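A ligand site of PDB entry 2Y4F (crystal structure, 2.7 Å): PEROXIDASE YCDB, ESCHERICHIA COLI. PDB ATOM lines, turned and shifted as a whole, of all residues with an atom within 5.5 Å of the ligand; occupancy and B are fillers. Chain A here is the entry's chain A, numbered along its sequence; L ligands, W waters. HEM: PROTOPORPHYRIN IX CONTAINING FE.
The backbone NH (N) of Thr 206 is in hydrogen-bond range of an oxygen (O1A) of the ligand, at 3.1 Å.
An oxygen (O2D) of the ligand lies within hydrogen-bond range of the side-chain amide nitrogen (ND2) of Asn 303 (2.6 Å).
The guanidinium group of Arg 316 lies within salt-bridge range of an oxygen (O1A) of the ligand (2.8 Å).
The backbone NH (N) of Ala 207 sits at hydrogen-bond distance from an oxygen (O2A) of the ligand, at 3.3 Å.
The guanidinium group (NH1) of Arg 305 lies within salt-bridge range of an oxygen (O1D) of the ligand (2.8 Å).
NE2 of His 298 binds FE of the ligand (2.2 Å).
An oxygen (O1A) of the ligand lies within hydrogen-bond range of the backbone NH (N) of Gly 205 (2.8 Å).
The backbone NH of Leu 200 lies within hydrogen-bond range of the side-chain amide oxygen of Asn 198 (3.0 Å).
The side-chain amide nitrogen (ND2) of Asn 208 lies within hydrogen-bond range of the backbone carbonyl oxygen (O) of Arg 316 (2.7 Å).
The guanidinium group (NH1) of Arg 316 is in salt-bridge range of the side-chain carboxylate (OD1) of Asp 204.
The backbone NH of Phe 202 is in hydrogen-bond range of the side-chain amide oxygen of Asn 198 (3.3 Å).
ND2 of Asn 303 lies close to NH1 of Arg 305.
N of Arg 242 sits at hydrogen-bond distance from O of Phe 337 (2.9 Å).
N of Leu 335 sits at hydrogen-bond distance from O of Ile 244.
Residues that only touch the ligand: Asn 198 (3.5 Å), Leu 200 (3.7 Å), Phe 202 (3.8 Å), Lys 203 (3.2 Å), Asp 204 (3.7 Å), Ile 244 (3.6 Å), Phe 246 (3.1 Å), Phe 263 (3.6 Å), Ile 299 (3.3 Å), Ala 302 (3.9 Å), Met 314 (3.5 Å), Leu 335 (3.5 Å), Phe 337 (3.4 Å), Phe 348 (3.5 Å), Val 351 (3.7 Å), Gln 352 (3.5 Å), Leu 355 (3.6 Å) and Leu 360 (3.97 Å).
25 residues have an atom within 4 Å of the ligand: Asn 198, Leu 200, Phe 202, Lys 203, Asp 204, Gly 205, Thr 206, Ala 207, Ile 244, Phe 246, Phe 263, His 298, Ile 299, Ala 302, Asn 303, Arg 305, Met 314, Arg 316, Leu 335, Phe 337, Phe 348, Val 351, Gln 352, Leu 355 and Leu 360.
The nearest printed residue that does not touch the ligand is Arg 265 (4.0002 Å).
Water W2 lies within hydrogen-bond range of OH of Tyr 284 (2.5 Å), O1D of the ligand (2.5 Å), NH1 of Arg 305 (2.7 Å), O of Asn 303 (3.0 Å) and O of Ile 299 (3.2 Å).
Water W3 lies within hydrogen-bond range of an oxygen (O2A) of the ligand (2.6 Å) and the guanidinium group of Arg 265 (2.9 Å).
Water W4 lies within hydrogen-bond range of OD1 of Asp 204 (3.1 Å) and NH1 of Arg 316 (3.2 Å).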
ATOM      1  N   ASN A 198     -14.246 -29.667   1.602  1.00  0.00           N
ATOM      2  CA  ASN A 198     -15.605 -30.039   1.214  1.00  0.00           C
ATOM      3  C   ASN A 198     -15.980 -31.487   1.586  1.00  0.00           C
ATOM      4  O   ASN A 198     -15.124 -32.255   2.043  1.00  0.00           O
ATOM      5  CB  ASN A 198     -15.897 -29.708  -0.250  1.00  0.00           C
ATOM      6  CG  ASN A 198     -15.295 -30.711  -1.213  1.00  0.00           C
ATOM      7  OD1 ASN A 198     -14.990 -31.832  -0.855  1.00  0.00           O
ATOM      8  ND2 ASN A 198     -15.149 -30.277  -2.456  1.00  0.00           N
ATOM      9  N   LEU A 200     -16.595 -34.153   0.071  1.00  0.00           N
ATOM     10  CA  LEU A 200     -15.960 -35.229  -0.627  1.00  0.00           C
ATOM     11  C   LEU A 200     -14.536 -35.389  -0.076  1.00  0.00           C
ATOM     12  O   LEU A 200     -13.781 -36.246  -0.538  1.00  0.00           O
ATOM     13  CB  LEU A 200     -15.922 -34.940  -2.110  1.00  0.00           C
ATOM     14  CG  LEU A 200     -17.215 -34.711  -2.917  1.00  0.00           C
ATOM     15  CD1 LEU A 200     -16.879 -34.316  -4.325  1.00  0.00           C
ATOM     16  CD2 LEU A 200     -18.152 -35.946  -2.898  1.00  0.00           C
ATOM     17  N   PHE A 202     -12.034 -33.192  -0.061  1.00  0.00           N
ATOM     18  CA  PHE A 202     -11.039 -32.401  -0.764  1.00  0.00           C
ATOM     19  C   PHE A 202     -11.033 -30.931  -0.315  1.00  0.00           C
ATOM     20  O   PHE A 202     -12.070 -30.357   0.028  1.00  0.00           O
ATOM     21  CB  PHE A 202     -11.283 -32.460  -2.276  1.00  0.00           C
ATOM     22  CG  PHE A 202     -10.690 -33.666  -2.953  1.00  0.00           C
ATOM     23  CD1 PHE A 202     -11.169 -34.937  -2.677  1.00  0.00           C
ATOM     24  CD2 PHE A 202      -9.668 -33.516  -3.886  1.00  0.00           C
ATOM     25  CE1 PHE A 202     -10.629 -36.054  -3.318  1.00  0.00           C
ATOM     26  CE2 PHE A 202      -9.114 -34.632  -4.525  1.00  0.00           C
ATOM     27  CZ  PHE A 202      -9.596 -35.898  -4.233  1.00  0.00           C
ATOM     28  N   LYS A 203      -9.845 -30.332  -0.337  1.00  0.00           N
ATOM     29  CA  LYS A 203      -9.668 -28.924  -0.099  1.00  0.00           C
ATOM     30  C   LYS A 203     -10.389 -28.153  -1.166  1.00  0.00           C
ATOM     31  O   LYS A 203     -10.181 -28.383  -2.360  1.00  0.00           O
ATOM     32  CB  LYS A 203      -8.189 -28.584  -0.083  1.00  0.00           C
ATOM     33  CG  LYS A 203      -7.597 -28.748   1.274  1.00  0.00           C
ATOM     34  CD  LYS A 203      -6.085 -28.740   1.231  1.00  0.00           C
ATOM     35  CE  LYS A 203      -5.556 -28.984   2.632  1.00  0.00           C
ATOM     36  NZ  LYS A 203      -4.522 -30.058   2.656  1.00  0.00           N
ATOM     37  N   ASP A 204     -11.249 -27.249  -0.735  1.00  0.00           N
ATOM     38  CA  ASP A 204     -12.055 -26.480  -1.652  1.00  0.00           C
ATOM     39  C   ASP A 204     -11.889 -24.998  -1.372  1.00  0.00           C
ATOM     40  O   ASP A 204     -12.411 -24.472  -0.380  1.00  0.00           O
ATOM     41  CB  ASP A 204     -13.528 -26.904  -1.527  1.00  0.00           C
ATOM     42  CG  ASP A 204     -14.420 -26.325  -2.640  1.00  0.00           C
ATOM     43  OD1 ASP A 204     -13.954 -25.419  -3.386  1.00  0.00           O
ATOM     44  OD2 ASP A 204     -15.595 -26.776  -2.757  1.00  0.00           O
ATOM     45  N   GLY A 205     -11.155 -24.325  -2.267  1.00  0.00           N
ATOM     46  CA  GLY A 205     -10.957 -22.872  -2.232  1.00  0.00           C
ATOM     47  C   GLY A 205      -9.583 -22.455  -2.757  1.00  0.00           C
ATOM     48  O   GLY A 205      -9.409 -21.331  -3.255  1.00  0.00           O
ATOM     49  N   THR A 206      -8.620 -23.378  -2.655  1.00  0.00           N
ATOM     50  CA  THR A 206      -7.199 -23.144  -2.919  1.00  0.00           C
ATOM     51  C   THR A 206      -6.884 -22.071  -3.941  1.00  0.00           C
ATOM     52  O   THR A 206      -6.147 -21.125  -3.627  1.00  0.00           O
ATOM     53  CB  THR A 206      -6.499 -24.466  -3.326  1.00  0.00           C
ATOM     54  OG1 THR A 206      -6.545 -25.355  -2.211  1.00  0.00           O
ATOM     55  CG2 THR A 206      -5.046 -24.239  -3.730  1.00  0.00           C
ATOM     56  N   ALA A 207      -7.425 -22.208  -5.153  1.00  0.00           N
ATOM     57  CA  ALA A 207      -6.973 -21.387  -6.269  1.00  0.00           C
ATOM     58  C   ALA A 207      -7.809 -20.150  -6.467  1.00  0.00           C
ATOM     59  O   ALA A 207      -7.626 -19.478  -7.459  1.00  0.00           O
ATOM     60  CB  ALA A 207      -6.911 -22.200  -7.550  1.00  0.00           C
ATOM     61  N   ASN A 208      -8.726 -19.878  -5.539  1.00  0.00           N
ATOM     62  CA  ASN A 208      -9.422 -18.576  -5.501  1.00  0.00           C
ATOM     63  C   ASN A 208      -8.468 -17.384  -5.639  1.00  0.00           C
ATOM     64  O   ASN A 208      -7.386 -17.354  -4.996  1.00  0.00           O
ATOM     65  CB  ASN A 208     -10.240 -18.400  -4.226  1.00  0.00           C
ATOM     66  CG  ASN A 208     -11.716 -18.672  -4.429  1.00  0.00           C
ATOM     67  OD1 ASN A 208     -12.248 -18.522  -5.523  1.00  0.00           O
ATOM     68  ND2 ASN A 208     -12.388 -19.052  -3.352  1.00  0.00           N
ATOM     69  N   ARG A 242     -25.493 -22.691  -7.278  1.00  0.00           N
ATOM     70  CA  ARG A 242     -25.917 -24.025  -7.675  1.00  0.00           C
ATOM     71  C   ARG A 242     -26.051 -24.949  -6.461  1.00  0.00           C
ATOM     72  O   ARG A 242     -25.140 -25.040  -5.646  1.00  0.00           O
ATOM     73  CB  ARG A 242     -24.928 -24.610  -8.691  1.00  0.00           C
ATOM     74  CG  ARG A 242     -24.679 -23.751  -9.885  1.00  0.00           C
ATOM     75  CD  ARG A 242     -25.674 -24.067 -10.974  1.00  0.00           C
ATOM     76  NE  ARG A 242     -25.190 -25.177 -11.783  1.00  0.00           N
ATOM     77  CZ  ARG A 242     -25.938 -25.911 -12.595  1.00  0.00           C
ATOM     78  NH1 ARG A 242     -27.247 -25.691 -12.728  1.00  0.00           N
ATOM     79  NH2 ARG A 242     -25.366 -26.898 -13.285  1.00  0.00           N
ATOM     80  N   ILE A 244     -26.131 -28.650  -5.291  1.00  0.00           N
ATOM     81  CA  ILE A 244     -25.510 -29.815  -5.931  1.00  0.00           C
ATOM     82  C   ILE A 244     -25.382 -30.986  -4.993  1.00  0.00           C
ATOM     83  O   ILE A 244     -24.660 -30.911  -4.004  1.00  0.00           O
ATOM     84  CB  ILE A 244     -24.109 -29.483  -6.466  1.00  0.00           C
ATOM     85  CG1 ILE A 244     -24.159 -28.229  -7.342  1.00  0.00           C
ATOM     86  CG2 ILE A 244     -23.568 -30.649  -7.259  1.00  0.00           C
ATOM     87  CD1 ILE A 244     -22.812 -27.656  -7.676  1.00  0.00           C
ATOM     88  N   PHE A 246     -24.180 -34.692  -3.784  1.00  0.00           N
ATOM     89  CA  PHE A 246     -23.075 -35.637  -3.943  1.00  0.00           C
ATOM     90  C   PHE A 246     -23.572 -37.068  -3.804  1.00  0.00           C
ATOM     91  O   PHE A 246     -24.318 -37.378  -2.887  1.00  0.00           O
ATOM     92  CB  PHE A 246     -21.984 -35.384  -2.888  1.00  0.00           C
ATOM     93  CG  PHE A 246     -21.355 -34.023  -2.984  1.00  0.00           C
ATOM     94  CD1 PHE A 246     -21.544 -33.221  -4.099  1.00  0.00           C
ATOM     95  CD2 PHE A 246     -20.543 -33.552  -1.957  1.00  0.00           C
ATOM     96  CE1 PHE A 246     -20.963 -31.978  -4.178  1.00  0.00           C
ATOM     97  CE2 PHE A 246     -19.946 -32.319  -2.043  1.00  0.00           C
ATOM     98  CZ  PHE A 246     -20.143 -31.535  -3.147  1.00  0.00           C
ATOM     99  N   PHE A 263     -10.490 -34.752  -9.801  1.00  0.00           N
ATOM    100  CA  PHE A 263     -10.155 -33.386  -9.431  1.00  0.00           C
ATOM    101  C   PHE A 263      -8.817 -32.924  -9.965  1.00  0.00           C
ATOM    102  O   PHE A 263      -8.626 -31.737 -10.184  1.00  0.00           O
ATOM    103  CB  PHE A 263     -10.162 -33.218  -7.912  1.00  0.00           C
ATOM    104  CG  PHE A 263     -11.503 -33.044  -7.351  1.00  0.00           C
ATOM    105  CD1 PHE A 263     -12.259 -31.910  -7.690  1.00  0.00           C
ATOM    106  CD2 PHE A 263     -12.060 -34.014  -6.527  1.00  0.00           C
ATOM    107  CE1 PHE A 263     -13.521 -31.748  -7.202  1.00  0.00           C
ATOM    108  CE2 PHE A 263     -13.343 -33.865  -6.039  1.00  0.00           C
ATOM    109  CZ  PHE A 263     -14.072 -32.735  -6.366  1.00  0.00           C
ATOM    110  N   ARG A 265      -6.012 -33.130  -8.113  1.00  0.00           N
ATOM    111  CA  ARG A 265      -5.194 -32.637  -7.006  1.00  0.00           C
ATOM    112  C   ARG A 265      -5.027 -33.705  -5.945  1.00  0.00           C
ATOM    113  O   ARG A 265      -5.927 -34.509  -5.720  1.00  0.00           O
ATOM    114  CB  ARG A 265      -5.817 -31.396  -6.371  1.00  0.00           C
ATOM    115  CG  ARG A 265      -5.376 -30.089  -7.031  1.00  0.00           C
ATOM    116  CD  ARG A 265      -6.040 -28.892  -6.360  1.00  0.00           C
ATOM    117  NE  ARG A 265      -5.606 -27.616  -6.943  1.00  0.00           N
ATOM    118  CZ  ARG A 265      -4.526 -26.927  -6.558  1.00  0.00           C
ATOM    119  NH1 ARG A 265      -3.733 -27.385  -5.596  1.00  0.00           N
ATOM    120  NH2 ARG A 265      -4.222 -25.790  -7.140  1.00  0.00           N
ATOM    121  N   PRO A 282      -0.340 -25.584 -11.343  1.00  0.00           N
ATOM    122  CA  PRO A 282      -0.149 -26.640 -12.333  1.00  0.00           C
ATOM    123  C   PRO A 282       0.486 -26.142 -13.630  1.00  0.00           C
ATOM    124  O   PRO A 282       0.305 -24.974 -14.009  1.00  0.00           O
ATOM    125  CB  PRO A 282      -1.569 -27.157 -12.588  1.00  0.00           C
ATOM    126  CG  PRO A 282      -2.476 -26.119 -12.049  1.00  0.00           C
ATOM    127  CD  PRO A 282      -1.746 -25.468 -10.924  1.00  0.00           C
ATOM    128  N   TYR A 284       0.239 -26.899 -17.269  1.00  0.00           N
ATOM    129  CA  TYR A 284      -0.511 -27.587 -18.312  1.00  0.00           C
ATOM    130  C   TYR A 284       0.260 -27.707 -19.616  1.00  0.00           C
ATOM    131  O   TYR A 284       0.181 -28.742 -20.277  1.00  0.00           O
ATOM    132  CB  TYR A 284      -1.892 -26.935 -18.545  1.00  0.00           C
ATOM    133  CG  TYR A 284      -2.816 -26.987 -17.345  1.00  0.00           C
ATOM    134  CD1 TYR A 284      -2.745 -28.045 -16.431  1.00  0.00           C
ATOM    135  CD2 TYR A 284      -3.783 -25.997 -17.130  1.00  0.00           C
ATOM    136  CE1 TYR A 284      -3.586 -28.109 -15.329  1.00  0.00           C
ATOM    137  CE2 TYR A 284      -4.630 -26.049 -16.033  1.00  0.00           C
ATOM    138  CZ  TYR A 284      -4.528 -27.111 -15.130  1.00  0.00           C
ATOM    139  OH  TYR A 284      -5.352 -27.179 -14.041  1.00  0.00           O
ATOM    140  N   HIS A 298     -11.419 -31.680 -13.123  1.00  0.00           N
ATOM    141  CA  HIS A 298     -12.191 -30.498 -12.758  1.00  0.00           C
ATOM    142  C   HIS A 298     -11.384 -29.188 -12.790  1.00  0.00           C
ATOM    143  O   HIS A 298     -11.843 -28.152 -13.274  1.00  0.00           O
ATOM    144  CB  HIS A 298     -12.832 -30.692 -11.383  1.00  0.00           C
ATOM    145  CG  HIS A 298     -13.622 -29.514 -10.922  1.00  0.00           C
ATOM    146  ND1 HIS A 298     -14.775 -29.114 -11.552  1.00  0.00           N
ATOM    147  CD2 HIS A 298     -13.428 -28.649  -9.905  1.00  0.00           C
ATOM    148  CE1 HIS A 298     -15.258 -28.052 -10.931  1.00  0.00           C
ATOM    149  NE2 HIS A 298     -14.464 -27.748  -9.921  1.00  0.00           N
ATOM    150  N   ILE A 299     -10.169 -29.277 -12.255  1.00  0.00           N
ATOM    151  CA  ILE A 299      -9.220 -28.182 -12.151  1.00  0.00           C
ATOM    152  C   ILE A 299      -8.796 -27.680 -13.553  1.00  0.00           C
ATOM    153  O   ILE A 299      -8.816 -26.473 -13.802  1.00  0.00           O
ATOM    154  CB  ILE A 299      -8.024 -28.673 -11.267  1.00  0.00           C
ATOM    155  CG1 ILE A 299      -7.000 -27.602 -10.980  1.00  0.00           C
ATOM    156  CG2 ILE A 299      -7.282 -29.849 -11.898  1.00  0.00           C
ATOM    157  CD1 ILE A 299      -5.798 -28.204 -10.255  1.00  0.00           C
ATOM    158  N   ALA A 302     -12.008 -26.304 -15.614  1.00  0.00           N
ATOM    159  CA  ALA A 302     -12.517 -25.088 -14.968  1.00  0.00           C
ATOM    160  C   ALA A 302     -11.601 -23.896 -15.137  1.00  0.00           C
ATOM    161  O   ALA A 302     -12.052 -22.749 -15.180  1.00  0.00           O
ATOM    162  CB  ALA A 302     -12.784 -25.335 -13.500  1.00  0.00           C
ATOM    163  N   ASN A 303     -10.309 -24.182 -15.208  1.00  0.00           N
ATOM    164  CA  ASN A 303      -9.284 -23.182 -15.380  1.00  0.00           C
ATOM    165  C   ASN A 303      -8.100 -23.816 -16.076  1.00  0.00           C
ATOM    166  O   ASN A 303      -7.277 -24.451 -15.434  1.00  0.00           O
ATOM    167  CB  ASN A 303      -8.851 -22.625 -14.030  1.00  0.00           C
ATOM    168  CG  ASN A 303      -7.806 -21.499 -14.140  1.00  0.00           C
ATOM    169  OD1 ASN A 303      -7.777 -20.713 -15.107  1.00  0.00           O
ATOM    170  ND2 ASN A 303      -6.954 -21.413 -13.122  1.00  0.00           N
ATOM    171  N   ARG A 305      -5.684 -22.256 -17.242  1.00  0.00           N
ATOM    172  CA  ARG A 305      -4.574 -21.312 -17.039  1.00  0.00           C
ATOM    173  C   ARG A 305      -3.916 -20.917 -18.360  1.00  0.00           C
ATOM    174  O   ARG A 305      -2.846 -21.426 -18.699  1.00  0.00           O
ATOM    175  CB  ARG A 305      -3.537 -21.910 -16.083  1.00  0.00           C
ATOM    176  CG  ARG A 305      -4.177 -22.710 -14.967  1.00  0.00           C
ATOM    177  CD  ARG A 305      -3.219 -23.129 -13.899  1.00  0.00           C
ATOM    178  NE  ARG A 305      -3.141 -22.143 -12.833  1.00  0.00           N
ATOM    179  CZ  ARG A 305      -3.865 -22.156 -11.712  1.00  0.00           C
ATOM    180  NH1 ARG A 305      -4.737 -23.126 -11.482  1.00  0.00           N
ATOM    181  NH2 ARG A 305      -3.711 -21.192 -10.815  1.00  0.00           N
ATOM    182  N   MET A 314     -13.196 -16.194 -11.072  1.00  0.00           N
ATOM    183  CA  MET A 314     -14.309 -15.831 -10.230  1.00  0.00           C
ATOM    184  C   MET A 314     -13.975 -16.137  -8.767  1.00  0.00           C
ATOM    185  O   MET A 314     -13.002 -16.832  -8.502  1.00  0.00           O
ATOM    186  CB  MET A 314     -15.507 -16.664 -10.641  1.00  0.00           C
ATOM    187  CG  MET A 314     -15.240 -18.150 -10.580  1.00  0.00           C
ATOM    188  SD  MET A 314     -16.556 -19.078 -11.348  1.00  0.00           S
ATOM    189  CE  MET A 314     -16.568 -20.445 -10.226  1.00  0.00           C
ATOM    190  N   ARG A 316     -15.088 -18.032  -5.454  1.00  0.00           N
ATOM    191  CA  ARG A 316     -15.968 -19.078  -4.967  1.00  0.00           C
ATOM    192  C   ARG A 316     -16.045 -18.976  -3.483  1.00  0.00           C
ATOM    193  O   ARG A 316     -15.040 -18.800  -2.803  1.00  0.00           O
ATOM    194  CB  ARG A 316     -15.496 -20.434  -5.420  1.00  0.00           C
ATOM    195  CG  ARG A 316     -15.674 -20.628  -6.912  1.00  0.00           C
ATOM    196  CD  ARG A 316     -14.936 -21.831  -7.437  1.00  0.00           C
ATOM    197  NE  ARG A 316     -13.504 -21.722  -7.226  1.00  0.00           N
ATOM    198  CZ  ARG A 316     -12.779 -22.561  -6.475  1.00  0.00           C
ATOM    199  NH1 ARG A 316     -13.381 -23.597  -5.862  1.00  0.00           N
ATOM    200  NH2 ARG A 316     -11.470 -22.381  -6.355  1.00  0.00           N
ATOM    201  N   LEU A 335     -22.885 -29.598  -1.911  1.00  0.00           N
ATOM    202  CA  LEU A 335     -22.352 -28.245  -1.838  1.00  0.00           C
ATOM    203  C   LEU A 335     -23.395 -27.170  -2.166  1.00  0.00           C
ATOM    204  O   LEU A 335     -24.116 -27.269  -3.148  1.00  0.00           O
ATOM    205  CB  LEU A 335     -21.226 -28.141  -2.854  1.00  0.00           C
ATOM    206  CG  LEU A 335     -20.560 -26.824  -3.218  1.00  0.00           C
ATOM    207  CD1 LEU A 335     -19.710 -26.336  -2.047  1.00  0.00           C
ATOM    208  CD2 LEU A 335     -19.697 -27.051  -4.450  1.00  0.00           C
ATOM    209  N   PHE A 337     -23.113 -24.053  -3.712  1.00  0.00           N
ATOM    210  CA  PHE A 337     -22.038 -23.442  -4.489  1.00  0.00           C
ATOM    211  C   PHE A 337     -22.401 -22.034  -4.840  1.00  0.00           C
ATOM    212  O   PHE A 337     -23.389 -21.799  -5.545  1.00  0.00           O
ATOM    213  CB  PHE A 337     -21.825 -24.189  -5.785  1.00  0.00           C
ATOM    214  CG  PHE A 337     -20.889 -23.488  -6.730  1.00  0.00           C
ATOM    215  CD1 PHE A 337     -21.373 -22.520  -7.611  1.00  0.00           C
ATOM    216  CD2 PHE A 337     -19.533 -23.795  -6.757  1.00  0.00           C
ATOM    217  CE1 PHE A 337     -20.507 -21.853  -8.478  1.00  0.00           C
ATOM    218  CE2 PHE A 337     -18.669 -23.133  -7.654  1.00  0.00           C
ATOM    219  CZ  PHE A 337     -19.166 -22.166  -8.500  1.00  0.00           C
ATOM    220  N   PHE A 348     -19.345 -17.550 -14.684  1.00  0.00           N
ATOM    221  CA  PHE A 348     -19.903 -18.888 -14.433  1.00  0.00           C
ATOM    222  C   PHE A 348     -20.283 -19.605 -15.721  1.00  0.00           C
ATOM    223  O   PHE A 348     -19.859 -20.736 -15.961  1.00  0.00           O
ATOM    224  CB  PHE A 348     -21.114 -18.832 -13.499  1.00  0.00           C
ATOM    225  CG  PHE A 348     -21.761 -20.180 -13.269  1.00  0.00           C
ATOM    226  CD1 PHE A 348     -21.309 -21.008 -12.248  1.00  0.00           C
ATOM    227  CD2 PHE A 348     -22.810 -20.615 -14.076  1.00  0.00           C
ATOM    228  CE1 PHE A 348     -21.884 -22.254 -12.043  1.00  0.00           C
ATOM    229  CE2 PHE A 348     -23.390 -21.844 -13.884  1.00  0.00           C
ATOM    230  CZ  PHE A 348     -22.931 -22.677 -12.866  1.00  0.00           C
ATOM    231  N   VAL A 351     -17.220 -20.960 -17.540  1.00  0.00           N
ATOM    232  CA  VAL A 351     -16.594 -22.079 -16.854  1.00  0.00           C
ATOM    233  C   VAL A 351     -17.447 -23.349 -16.887  1.00  0.00           C
ATOM    234  O   VAL A 351     -16.901 -24.448 -17.021  1.00  0.00           O
ATOM    235  CB  VAL A 351     -16.232 -21.731 -15.382  1.00  0.00           C
ATOM    236  CG1 VAL A 351     -15.435 -22.865 -14.719  1.00  0.00           C
ATOM    237  CG2 VAL A 351     -15.420 -20.446 -15.318  1.00  0.00           C
ATOM    238  N   GLN A 352     -18.764 -23.223 -16.763  1.00  0.00           N
ATOM    239  CA  GLN A 352     -19.616 -24.424 -16.782  1.00  0.00           C
ATOM    240  C   GLN A 352     -19.704 -25.056 -18.188  1.00  0.00           C
ATOM    241  O   GLN A 352     -19.764 -26.287 -18.324  1.00  0.00           O
ATOM    242  CB  GLN A 352     -21.006 -24.137 -16.218  1.00  0.00           C
ATOM    243  CG  GLN A 352     -21.878 -25.378 -16.042  1.00  0.00           C
ATOM    244  CD  GLN A 352     -21.396 -26.346 -14.958  1.00  0.00           C
ATOM    245  OE1 GLN A 352     -21.116 -27.523 -15.230  1.00  0.00           O
ATOM    246  NE2 GLN A 352     -21.304 -25.872 -13.735  1.00  0.00           N
ATOM    247  N   LEU A 355     -16.935 -27.174 -18.278  1.00  0.00           N
ATOM    248  CA  LEU A 355     -17.034 -28.275 -17.333  1.00  0.00           C
ATOM    249  C   LEU A 355     -17.989 -29.373 -17.795  1.00  0.00           C
ATOM    250  O   LEU A 355     -17.977 -30.488 -17.250  1.00  0.00           O
ATOM    251  CB  LEU A 355     -17.461 -27.759 -15.955  1.00  0.00           C
ATOM    252  CG  LEU A 355     -16.419 -27.065 -15.091  1.00  0.00           C
ATOM    253  CD1 LEU A 355     -17.089 -26.459 -13.858  1.00  0.00           C
ATOM    254  CD2 LEU A 355     -15.285 -28.044 -14.689  1.00  0.00           C
ATOM    255  N   LEU A 360     -16.273 -35.552 -12.947  1.00  0.00           N
ATOM    256  CA  LEU A 360     -17.026 -35.366 -11.717  1.00  0.00           C
ATOM    257  C   LEU A 360     -18.544 -35.578 -11.869  1.00  0.00           C
ATOM    258  O   LEU A 360     -19.217 -35.977 -10.933  1.00  0.00           O
ATOM    259  CB  LEU A 360     -16.735 -33.960 -11.160  1.00  0.00           C
ATOM    260  CG  LEU A 360     -17.093 -33.657  -9.717  1.00  0.00           C
ATOM    261  CD1 LEU A 360     -16.448 -34.682  -8.804  1.00  0.00           C
ATOM    262  CD2 LEU A 360     -16.690 -32.247  -9.342  1.00  0.00           C
ATOM    263  N   VAL A 364     -21.822 -35.975  -8.985  1.00  0.00           N
ATOM    264  CA  VAL A 364     -22.585 -34.800  -8.548  1.00  0.00           C
ATOM    265  C   VAL A 364     -23.842 -34.568  -9.398  1.00  0.00           C
ATOM    266  O   VAL A 364     -23.865 -34.872 -10.607  1.00  0.00           O
ATOM    267  CB  VAL A 364     -21.722 -33.529  -8.525  1.00  0.00           C
ATOM    268  CG1 VAL A 364     -20.490 -33.745  -7.667  1.00  0.00           C
ATOM    269  CG2 VAL A 364     -21.341 -33.115  -9.950  1.00  0.00           C
HETATM  270  CHA HEM L   1     -11.679 -25.760  -7.996  1.00  0.00           C
HETATM  271  CHB HEM L   1     -14.692 -28.726  -5.725  1.00  0.00           C
HETATM  272  CHC HEM L   1     -18.134 -27.252  -8.746  1.00  0.00           C
HETATM  273  CHD HEM L   1     -15.303 -23.785 -10.538  1.00  0.00           C
HETATM  274  C1A HEM L   1     -12.185 -26.766  -7.207  1.00  0.00           C
HETATM  275  C2A HEM L   1     -11.380 -27.660  -6.410  1.00  0.00           C
HETATM  276  C3A HEM L   1     -12.212 -28.476  -5.766  1.00  0.00           C
HETATM  277  C4A HEM L   1     -13.551 -28.125  -6.157  1.00  0.00           C
HETATM  278  CMA HEM L   1     -11.880 -29.599  -4.772  1.00  0.00           C
HETATM  279  CAA HEM L   1      -9.830 -27.613  -6.316  1.00  0.00           C
HETATM  280  CBA HEM L   1      -9.354 -26.673  -5.212  1.00  0.00           C
HETATM  281  CGA HEM L   1      -9.553 -25.228  -5.598  1.00  0.00           C
HETATM  282  O1A HEM L   1     -10.327 -24.517  -4.920  1.00  0.00           O
HETATM  283  O2A HEM L   1      -8.949 -24.768  -6.599  1.00  0.00           O
HETATM  284  C1B HEM L   1     -15.861 -28.649  -6.426  1.00  0.00           C
HETATM  285  C2B HEM L   1     -16.967 -29.570  -6.308  1.00  0.00           C
HETATM  286  C3B HEM L   1     -17.907 -29.167  -7.157  1.00  0.00           C
HETATM  287  C4B HEM L   1     -17.431 -27.968  -7.830  1.00  0.00           C
HETATM  288  CMB HEM L   1     -16.990 -30.806  -5.391  1.00  0.00           C
HETATM  289  CAB HEM L   1     -19.264 -29.855  -7.406  1.00  0.00           C
HETATM  290  CBB HEM L   1     -20.117 -29.947  -6.389  1.00  0.00           C
HETATM  291  C1C HEM L   1     -17.703 -26.153  -9.426  1.00  0.00           C
HETATM  292  C2C HEM L   1     -18.521 -25.333 -10.294  1.00  0.00           C
HETATM  293  C3C HEM L   1     -17.719 -24.371 -10.807  1.00  0.00           C
HETATM  294  C4C HEM L   1     -16.390 -24.570 -10.275  1.00  0.00           C
HETATM  295  CMC HEM L   1     -20.021 -25.542 -10.542  1.00  0.00           C
HETATM  296  CAC HEM L   1     -18.094 -23.216 -11.770  1.00  0.00           C
HETATM  297  CBC HEM L   1     -18.689 -23.414 -12.948  1.00  0.00           C
HETATM  298  C1D HEM L   1     -14.051 -23.975 -10.024  1.00  0.00           C
HETATM  299  C2D HEM L   1     -12.898 -23.157 -10.302  1.00  0.00           C
HETATM  300  C3D HEM L   1     -11.774 -23.788  -9.498  1.00  0.00           C
HETATM  301  C4D HEM L   1     -12.376 -24.912  -8.824  1.00  0.00           C
HETATM  302  CMD HEM L   1     -12.784 -21.906 -11.206  1.00  0.00           C
HETATM  303  CAD HEM L   1     -10.302 -23.339  -9.426  1.00  0.00           C
HETATM  304  CBD HEM L   1      -9.461 -24.346 -10.204  1.00  0.00           C
HETATM  305  CGD HEM L   1      -8.204 -23.693 -10.693  1.00  0.00           C
HETATM  306  O1D HEM L   1      -7.117 -24.321 -10.589  1.00  0.00           O
HETATM  307  O2D HEM L   1      -8.276 -22.541 -11.194  1.00  0.00           O
HETATM  308  NA  HEM L   1     -13.504 -27.074  -7.046  1.00  0.00           N
HETATM  309  NB  HEM L   1     -16.177 -27.683  -7.359  1.00  0.00           N
HETATM  310  NC  HEM L   1     -16.413 -25.671  -9.433  1.00  0.00           N
HETATM  311  ND  HEM L   1     -13.716 -24.990  -9.151  1.00  0.00           N
HETATM  312 FE   HEM L   1     -14.931 -26.362  -8.253  1.00  0.00          FE
HETATM  313  O   HOH W   1     -12.092 -19.878 -13.595  1.00  0.00           O
HETATM  314  O   HOH W   2      -6.094 -25.139 -12.752  1.00  0.00           O
HETATM  315  O   HOH W   3      -7.275 -25.731  -8.356  1.00  0.00           O
HETATM  316  O   HOH W   4     -16.104 -25.209  -5.667  1.00  0.00           O
